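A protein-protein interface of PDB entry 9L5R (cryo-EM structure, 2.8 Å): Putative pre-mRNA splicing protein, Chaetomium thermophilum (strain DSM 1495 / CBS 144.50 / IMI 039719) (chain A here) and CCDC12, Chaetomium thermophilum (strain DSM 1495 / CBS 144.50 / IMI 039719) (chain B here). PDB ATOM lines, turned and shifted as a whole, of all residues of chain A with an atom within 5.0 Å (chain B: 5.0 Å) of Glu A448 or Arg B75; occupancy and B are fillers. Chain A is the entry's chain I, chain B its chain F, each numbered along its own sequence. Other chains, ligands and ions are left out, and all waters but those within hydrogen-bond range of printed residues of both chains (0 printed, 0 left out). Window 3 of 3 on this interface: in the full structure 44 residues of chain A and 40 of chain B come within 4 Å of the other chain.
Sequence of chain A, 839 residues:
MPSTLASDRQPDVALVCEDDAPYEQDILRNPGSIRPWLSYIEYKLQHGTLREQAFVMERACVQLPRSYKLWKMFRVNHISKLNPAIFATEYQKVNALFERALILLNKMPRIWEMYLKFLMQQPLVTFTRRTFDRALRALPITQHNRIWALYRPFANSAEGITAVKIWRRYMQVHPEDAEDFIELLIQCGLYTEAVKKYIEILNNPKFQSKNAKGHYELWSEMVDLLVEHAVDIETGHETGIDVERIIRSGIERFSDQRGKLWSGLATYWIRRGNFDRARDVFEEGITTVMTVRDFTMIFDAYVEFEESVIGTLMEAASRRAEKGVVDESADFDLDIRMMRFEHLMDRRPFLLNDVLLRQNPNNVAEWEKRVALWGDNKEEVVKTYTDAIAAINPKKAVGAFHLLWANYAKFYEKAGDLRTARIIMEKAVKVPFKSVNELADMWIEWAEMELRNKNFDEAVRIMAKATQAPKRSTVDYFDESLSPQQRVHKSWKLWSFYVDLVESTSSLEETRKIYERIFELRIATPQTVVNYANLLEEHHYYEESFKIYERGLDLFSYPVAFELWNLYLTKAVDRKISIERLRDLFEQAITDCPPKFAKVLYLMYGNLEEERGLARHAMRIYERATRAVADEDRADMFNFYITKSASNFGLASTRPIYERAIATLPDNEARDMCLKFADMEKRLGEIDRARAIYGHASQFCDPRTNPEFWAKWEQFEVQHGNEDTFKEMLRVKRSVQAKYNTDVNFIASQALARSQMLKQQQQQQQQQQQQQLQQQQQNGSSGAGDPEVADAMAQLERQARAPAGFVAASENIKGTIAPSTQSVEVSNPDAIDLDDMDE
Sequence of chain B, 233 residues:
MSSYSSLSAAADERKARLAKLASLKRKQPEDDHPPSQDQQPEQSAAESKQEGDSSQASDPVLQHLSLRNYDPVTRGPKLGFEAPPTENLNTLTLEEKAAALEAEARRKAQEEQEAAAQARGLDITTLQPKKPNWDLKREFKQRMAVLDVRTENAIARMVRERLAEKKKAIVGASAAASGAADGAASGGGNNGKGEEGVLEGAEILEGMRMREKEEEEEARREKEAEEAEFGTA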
ATOM      1  N   ASP A 441       1.984 -25.442  10.754  1.00  0.00           N
ATOM      2  CA  ASP A 441       0.790 -25.289   9.941  1.00  0.00           C
ATOM      3  C   ASP A 441       0.278 -26.636   9.453  1.00  0.00           C
ATOM      4  O   ASP A 441      -0.933 -26.852   9.393  1.00  0.00           O
ATOM      5  CB  ASP A 441       1.070 -24.346   8.774  1.00  0.00           C
ATOM      6  CG  ASP A 441       1.071 -22.890   9.199  1.00  0.00           C
ATOM      7  OD1 ASP A 441       0.321 -22.550  10.138  1.00  0.00           O
ATOM      8  OD2 ASP A 441       1.819 -22.087   8.602  1.00  0.00           O
ATOM      9  N   ILE A 444      -1.447 -28.377  12.546  1.00  0.00           N
ATOM     10  CA  ILE A 444      -2.762 -27.808  12.803  1.00  0.00           C
ATOM     11  C   ILE A 444      -3.705 -28.040  11.630  1.00  0.00           C
ATOM     12  O   ILE A 444      -4.920 -28.049  11.827  1.00  0.00           O
ATOM     13  CB  ILE A 444      -2.691 -26.311  13.160  1.00  0.00           C
ATOM     14  CG1 ILE A 444      -2.309 -25.466  11.948  1.00  0.00           C
ATOM     15  CG2 ILE A 444      -1.734 -26.078  14.315  1.00  0.00           C
ATOM     16  CD1 ILE A 444      -2.614 -23.996  12.108  1.00  0.00           C
ATOM     17  N   GLU A 445      -3.185 -28.271  10.419  1.00  0.00           N
ATOM     18  CA  GLU A 445      -4.053 -28.653   9.310  1.00  0.00           C
ATOM     19  C   GLU A 445      -4.639 -30.042   9.521  1.00  0.00           C
ATOM     20  O   GLU A 445      -5.818 -30.269   9.234  1.00  0.00           O
ATOM     21  CB  GLU A 445      -3.288 -28.595   7.989  1.00  0.00           C
ATOM     22  CG  GLU A 445      -3.343 -27.242   7.293  1.00  0.00           C
ATOM     23  CD  GLU A 445      -4.757 -26.791   6.995  1.00  0.00           C
ATOM     24  OE1 GLU A 445      -5.575 -27.627   6.560  1.00  0.00           O
ATOM     25  OE2 GLU A 445      -5.052 -25.595   7.198  1.00  0.00           O
ATOM     26  N   TRP A 446      -3.828 -30.979  10.020  1.00  0.00           N
ATOM     27  CA  TRP A 446      -4.347 -32.302  10.368  1.00  0.00           C
ATOM     28  C   TRP A 446      -5.415 -32.207  11.451  1.00  0.00           C
ATOM     29  O   TRP A 446      -6.480 -32.842  11.352  1.00  0.00           O
ATOM     30  CB  TRP A 446      -3.202 -33.205  10.832  1.00  0.00           C
ATOM     31  CG  TRP A 446      -3.519 -34.675  10.832  1.00  0.00           C
ATOM     32  CD1 TRP A 446      -4.706 -35.260  10.504  1.00  0.00           C
ATOM     33  CD2 TRP A 446      -2.623 -35.745  11.158  1.00  0.00           C
ATOM     34  NE1 TRP A 446      -4.606 -36.624  10.605  1.00  0.00           N
ATOM     35  CE2 TRP A 446      -3.333 -36.949  10.993  1.00  0.00           C
ATOM     36  CE3 TRP A 446      -1.282 -35.803  11.541  1.00  0.00           C
ATOM     37  CZ2 TRP A 446      -2.758 -38.194  11.234  1.00  0.00           C
ATOM     38  CZ3 TRP A 446      -0.711 -37.042  11.775  1.00  0.00           C
ATOM     39  CH2 TRP A 446      -1.449 -38.220  11.620  1.00  0.00           C
ATOM     40  N   ALA A 447      -5.149 -31.407  12.487  1.00  0.00           N
ATOM     41  CA  ALA A 447      -6.125 -31.243  13.561  1.00  0.00           C
ATOM     42  C   ALA A 447      -7.406 -30.591  13.056  1.00  0.00           C
ATOM     43  O   ALA A 447      -8.510 -30.995  13.441  1.00  0.00           O
ATOM     44  CB  ALA A 447      -5.525 -30.426  14.697  1.00  0.00           C
ATOM     45  N   GLU A 448      -7.278 -29.593  12.179  1.00  0.00           N
ATOM     46  CA  GLU A 448      -8.445 -28.935  11.608  1.00  0.00           C
ATOM     47  C   GLU A 448      -9.225 -29.881  10.709  1.00  0.00           C
ATOM     48  O   GLU A 448     -10.454 -29.802  10.643  1.00  0.00           O
ATOM     49  CB  GLU A 448      -8.014 -27.698  10.826  1.00  0.00           C
ATOM     50  CG  GLU A 448      -7.852 -26.457  11.676  1.00  0.00           C
ATOM     51  CD  GLU A 448      -6.982 -25.414  11.008  1.00  0.00           C
ATOM     52  OE1 GLU A 448      -6.553 -25.648   9.859  1.00  0.00           O
ATOM     53  OE2 GLU A 448      -6.724 -24.363  11.631  1.00  0.00           O
ATOM     54  N   MET A 449      -8.529 -30.788  10.018  1.00  0.00           N
ATOM     55  CA  MET A 449      -9.202 -31.759   9.162  1.00  0.00           C
ATOM     56  C   MET A 449     -10.064 -32.708   9.986  1.00  0.00           C
ATOM     57  O   MET A 449     -11.240 -32.931   9.666  1.00  0.00           O
ATOM     58  CB  MET A 449      -8.165 -32.541   8.359  1.00  0.00           C
ATOM     59  CG  MET A 449      -8.754 -33.488   7.348  1.00  0.00           C
ATOM     60  SD  MET A 449      -9.657 -32.553   6.107  1.00  0.00           S
ATOM     61  CE  MET A 449      -8.294 -31.814   5.214  1.00  0.00           C
ATOM     62  N   GLU A 450      -9.492 -33.262  11.062  1.00  0.00           N
ATOM     63  CA  GLU A 450     -10.268 -34.137  11.942  1.00  0.00           C
ATOM     64  C   GLU A 450     -11.415 -33.383  12.605  1.00  0.00           C
ATOM     65  O   GLU A 450     -12.532 -33.910  12.733  1.00  0.00           O
ATOM     66  CB  GLU A 450      -9.360 -34.756  13.001  1.00  0.00           C
ATOM     67  CG  GLU A 450      -8.144 -35.451  12.436  1.00  0.00           C
ATOM     68  CD  GLU A 450      -8.465 -36.805  11.851  1.00  0.00           C
ATOM     69  OE1 GLU A 450      -9.338 -37.500  12.408  1.00  0.00           O
ATOM     70  OE2 GLU A 450      -7.844 -37.176  10.835  1.00  0.00           O
ATOM     71  N   LEU A 451     -11.158 -32.143  13.021  1.00  0.00           N
ATOM     72  CA  LEU A 451     -12.189 -31.322  13.637  1.00  0.00           C
ATOM     73  C   LEU A 451     -13.301 -30.984  12.650  1.00  0.00           C
ATOM     74  O   LEU A 451     -14.452 -30.791  13.055  1.00  0.00           O
ATOM     75  CB  LEU A 451     -11.541 -30.055  14.192  1.00  0.00           C
ATOM     76  CG  LEU A 451     -12.237 -29.274  15.297  1.00  0.00           C
ATOM     77  CD1 LEU A 451     -12.295 -30.108  16.554  1.00  0.00           C
ATOM     78  CD2 LEU A 451     -11.470 -28.006  15.554  1.00  0.00           C
ATOM     79  N   ARG A 452     -12.971 -30.897  11.359  1.00  0.00           N
ATOM     80  CA  ARG A 452     -13.992 -30.728  10.332  1.00  0.00           C
ATOM     81  C   ARG A 452     -14.843 -31.984  10.200  1.00  0.00           C
ATOM     82  O   ARG A 452     -16.076 -31.915  10.243  1.00  0.00           O
ATOM     83  CB  ARG A 452     -13.335 -30.375   8.999  1.00  0.00           C
ATOM     84  CG  ARG A 452     -13.020 -28.900   8.836  1.00  0.00           C
ATOM     85  CD  ARG A 452     -13.241 -28.452   7.409  1.00  0.00           C
ATOM     86  NE  ARG A 452     -12.800 -29.465   6.459  1.00  0.00           N
ATOM     87  CZ  ARG A 452     -11.653 -29.423   5.796  1.00  0.00           C
ATOM     88  NH1 ARG A 452     -10.788 -28.437   5.973  1.00  0.00           N
ATOM     89  NH2 ARG A 452     -11.365 -30.395   4.936  1.00  0.00           N
ATOM     90  N   LYS A 493       2.526 -22.049  18.731  1.00  0.00           N
ATOM     91  CA  LYS A 493       1.278 -22.151  17.982  1.00  0.00           C
ATOM     92  C   LYS A 493       0.545 -23.446  18.320  1.00  0.00           C
ATOM     93  O   LYS A 493      -0.654 -23.432  18.641  1.00  0.00           O
ATOM     94  CB  LYS A 493       1.578 -22.068  16.487  1.00  0.00           C
ATOM     95  CG  LYS A 493       0.367 -21.975  15.602  1.00  0.00           C
ATOM     96  CD  LYS A 493       0.784 -21.897  14.146  1.00  0.00           C
ATOM     97  CE  LYS A 493       1.494 -20.588  13.852  1.00  0.00           C
ATOM     98  NZ  LYS A 493       1.816 -20.439  12.409  1.00  0.00           N
ATOM     99  N   PHE A 497      -3.057 -23.854  20.429  1.00  0.00           N
ATOM    100  CA  PHE A 497      -4.139 -24.604  19.798  1.00  0.00           C
ATOM    101  C   PHE A 497      -4.543 -25.808  20.639  1.00  0.00           C
ATOM    102  O   PHE A 497      -5.733 -26.055  20.852  1.00  0.00           O
ATOM    103  CB  PHE A 497      -3.702 -25.046  18.401  1.00  0.00           C
ATOM    104  CG  PHE A 497      -4.788 -25.683  17.592  1.00  0.00           C
ATOM    105  CD1 PHE A 497      -5.601 -24.913  16.784  1.00  0.00           C
ATOM    106  CD2 PHE A 497      -4.986 -27.054  17.621  1.00  0.00           C
ATOM    107  CE1 PHE A 497      -6.601 -25.493  16.034  1.00  0.00           C
ATOM    108  CE2 PHE A 497      -5.986 -27.636  16.880  1.00  0.00           C
ATOM    109  CZ  PHE A 497      -6.792 -26.856  16.082  1.00  0.00           C
ATOM    110  N   VAL B  61     -14.381 -25.188  13.845  1.00  0.00           N
ATOM    111  CA  VAL B  61     -13.135 -24.888  14.543  1.00  0.00           C
ATOM    112  C   VAL B  61     -13.361 -23.818  15.605  1.00  0.00           C
ATOM    113  O   VAL B  61     -12.940 -23.962  16.759  1.00  0.00           O
ATOM    114  CB  VAL B  61     -12.053 -24.469  13.533  1.00  0.00           C
ATOM    115  CG1 VAL B  61     -10.782 -24.054  14.251  1.00  0.00           C
ATOM    116  CG2 VAL B  61     -11.782 -25.601  12.556  1.00  0.00           C
ATOM    117  N   TYR B  70      -5.814 -19.186  21.630  1.00  0.00           N
ATOM    118  CA  TYR B  70      -5.669 -19.255  20.187  1.00  0.00           C
ATOM    119  C   TYR B  70      -6.392 -18.096  19.519  1.00  0.00           C
ATOM    120  O   TYR B  70      -7.476 -17.691  19.946  1.00  0.00           O
ATOM    121  CB  TYR B  70      -6.207 -20.583  19.658  1.00  0.00           C
ATOM    122  CG  TYR B  70      -5.878 -20.844  18.212  1.00  0.00           C
ATOM    123  CD1 TYR B  70      -4.658 -21.385  17.847  1.00  0.00           C
ATOM    124  CD2 TYR B  70      -6.796 -20.563  17.211  1.00  0.00           C
ATOM    125  CE1 TYR B  70      -4.355 -21.627  16.526  1.00  0.00           C
ATOM    126  CE2 TYR B  70      -6.502 -20.802  15.889  1.00  0.00           C
ATOM    127  CZ  TYR B  70      -5.282 -21.334  15.552  1.00  0.00           C
ATOM    128  OH  TYR B  70      -4.986 -21.575  14.232  1.00  0.00           O
ATOM    129  N   ASP B  71      -5.774 -17.559  18.472  1.00  0.00           N
ATOM    130  CA  ASP B  71      -6.370 -16.507  17.670  1.00  0.00           C
ATOM    131  C   ASP B  71      -6.655 -17.053  16.281  1.00  0.00           C
ATOM    132  O   ASP B  71      -5.713 -17.432  15.569  1.00  0.00           O
ATOM    133  CB  ASP B  71      -5.444 -15.300  17.594  1.00  0.00           C
ATOM    134  CG  ASP B  71      -6.131 -14.075  17.049  1.00  0.00           C
ATOM    135  OD1 ASP B  71      -6.855 -13.410  17.814  1.00  0.00           O
ATOM    136  OD2 ASP B  71      -5.939 -13.774  15.855  1.00  0.00           O
ATOM    137  N   PRO B  72      -7.913 -17.114  15.854  1.00  0.00           N
ATOM    138  CA  PRO B  72      -8.236 -17.822  14.611  1.00  0.00           C
ATOM    139  C   PRO B  72      -7.999 -17.003  13.352  1.00  0.00           C
ATOM    140  O   PRO B  72      -7.729 -17.569  12.289  1.00  0.00           O
ATOM    141  CB  PRO B  72      -9.719 -18.153  14.791  1.00  0.00           C
ATOM    142  CG  PRO B  72     -10.242 -17.023  15.613  1.00  0.00           C
ATOM    143  CD  PRO B  72      -9.109 -16.537  16.489  1.00  0.00           C
ATOM    144  N   VAL B  73      -8.099 -15.675  13.450  1.00  0.00           N
ATOM    145  CA  VAL B  73      -7.918 -14.843  12.268  1.00  0.00           C
ATOM    146  C   VAL B  73      -6.444 -14.708  11.900  1.00  0.00           C
ATOM    147  O   VAL B  73      -6.124 -14.427  10.739  1.00  0.00           O
ATOM    148  CB  VAL B  73      -8.592 -13.473  12.481  1.00  0.00           C
ATOM    149  CG1 VAL B  73      -7.797 -12.601  13.437  1.00  0.00           C
ATOM    150  CG2 VAL B  73      -8.835 -12.759  11.153  1.00  0.00           C
ATOM    151  N   THR B  74      -5.535 -14.938  12.844  1.00  0.00           N
ATOM    152  CA  THR B  74      -4.105 -14.910  12.570  1.00  0.00           C
ATOM    153  C   THR B  74      -3.477 -16.295  12.579  1.00  0.00           C
ATOM    154  O   THR B  74      -2.279 -16.412  12.297  1.00  0.00           O
ATOM    155  CB  THR B  74      -3.385 -14.017  13.584  1.00  0.00           C
ATOM    156  OG1 THR B  74      -3.620 -14.511  14.907  1.00  0.00           O
ATOM    157  CG2 THR B  74      -3.888 -12.587  13.481  1.00  0.00           C
ATOM    158  N   ARG B  75      -4.260 -17.332  12.896  1.00  0.00           N
ATOM    159  CA  ARG B  75      -3.809 -18.728  12.934  1.00  0.00           C
ATOM    160  C   ARG B  75      -2.624 -18.918  13.877  1.00  0.00           C
ATOM    161  O   ARG B  75      -1.681 -19.651  13.579  1.00  0.00           O
ATOM    162  CB  ARG B  75      -3.473 -19.246  11.532  1.00  0.00           C
ATOM    163  CG  ARG B  75      -4.686 -19.486  10.655  1.00  0.00           C
ATOM    164  CD  ARG B  75      -4.312 -20.274   9.412  1.00  0.00           C
ATOM    165  NE  ARG B  75      -5.489 -20.772   8.711  1.00  0.00           N
ATOM    166  CZ  ARG B  75      -6.160 -21.860   9.060  1.00  0.00           C
ATOM    167  NH1 ARG B  75      -5.796 -22.595  10.098  1.00  0.00           N
ATOM    168  NH2 ARG B  75      -7.223 -22.223   8.348  1.00  0.00           N
ATOM    169  N   GLY B  76      -2.675 -18.251  15.026  1.00  0.00           N
ATOM    170  CA  GLY B  76      -1.611 -18.331  15.996  1.00  0.00           C
ATOM    171  C   GLY B  76      -2.087 -17.991  17.391  1.00  0.00           C
ATOM    172  O   GLY B  76      -3.285 -17.836  17.641  1.00  0.00           O
ATOM    173  N   PRO B  77      -1.154 -17.879  18.331  1.00  0.00           N
ATOM    174  CA  PRO B  77      -1.526 -17.536  19.706  1.00  0.00           C
ATOM    175  C   PRO B  77      -2.009 -16.100  19.828  1.00  0.00           C
ATOM    176  O   PRO B  77      -1.641 -15.224  19.045  1.00  0.00           O
ATOM    177  CB  PRO B  77      -0.225 -17.746  20.483  1.00  0.00           C
ATOM    178  CG  PRO B  77       0.834 -17.526  19.473  1.00  0.00           C
ATOM    179  CD  PRO B  77       0.297 -18.070  18.187  1.00  0.00           C
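NZ of Lys A493 lies within salt-bridge range of OD1 of Asp A441.
Of the printed residues of chain A, Arg B75 touches Glu A448 and Lys A493.
Of the printed residues of chain B, Leu A451 touches Val B61 (3.7 Å).
Of the printed residues of chain A, Val B61 touches Leu A451.
Of the printed residues of chain B, Lys A493 touches Arg B75 (3.3 Å).
Printed residues of chain B within 4 Å of Phe A497: Tyr B70.
The nearest printed residue of chain A that does not touch Tyr B70 is Glu A448 (4.2 Å).
The side-chain carboxylate (OE2) of Glu A448 lies within salt-bridge range of the guanidinium group (NH1) of Arg B75 (2.5 Å).
Among the printed residues, Asp or Glu carboxylates within 4 Å of a Lys or Arg side-chain nitrogen of the other chain: Glu A448 with Arg B75 (2.5 Å).
Tyr B70 touches Ile A444 (OH to CD1, 3.9999 Å).
Leu A451 touches Val B61.
O of Arg B75 touches CE of Lys A493, 3.3 Å away.
Tyr B70 touches Phe A497 (CE1 to CD1, 3.5 Å).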
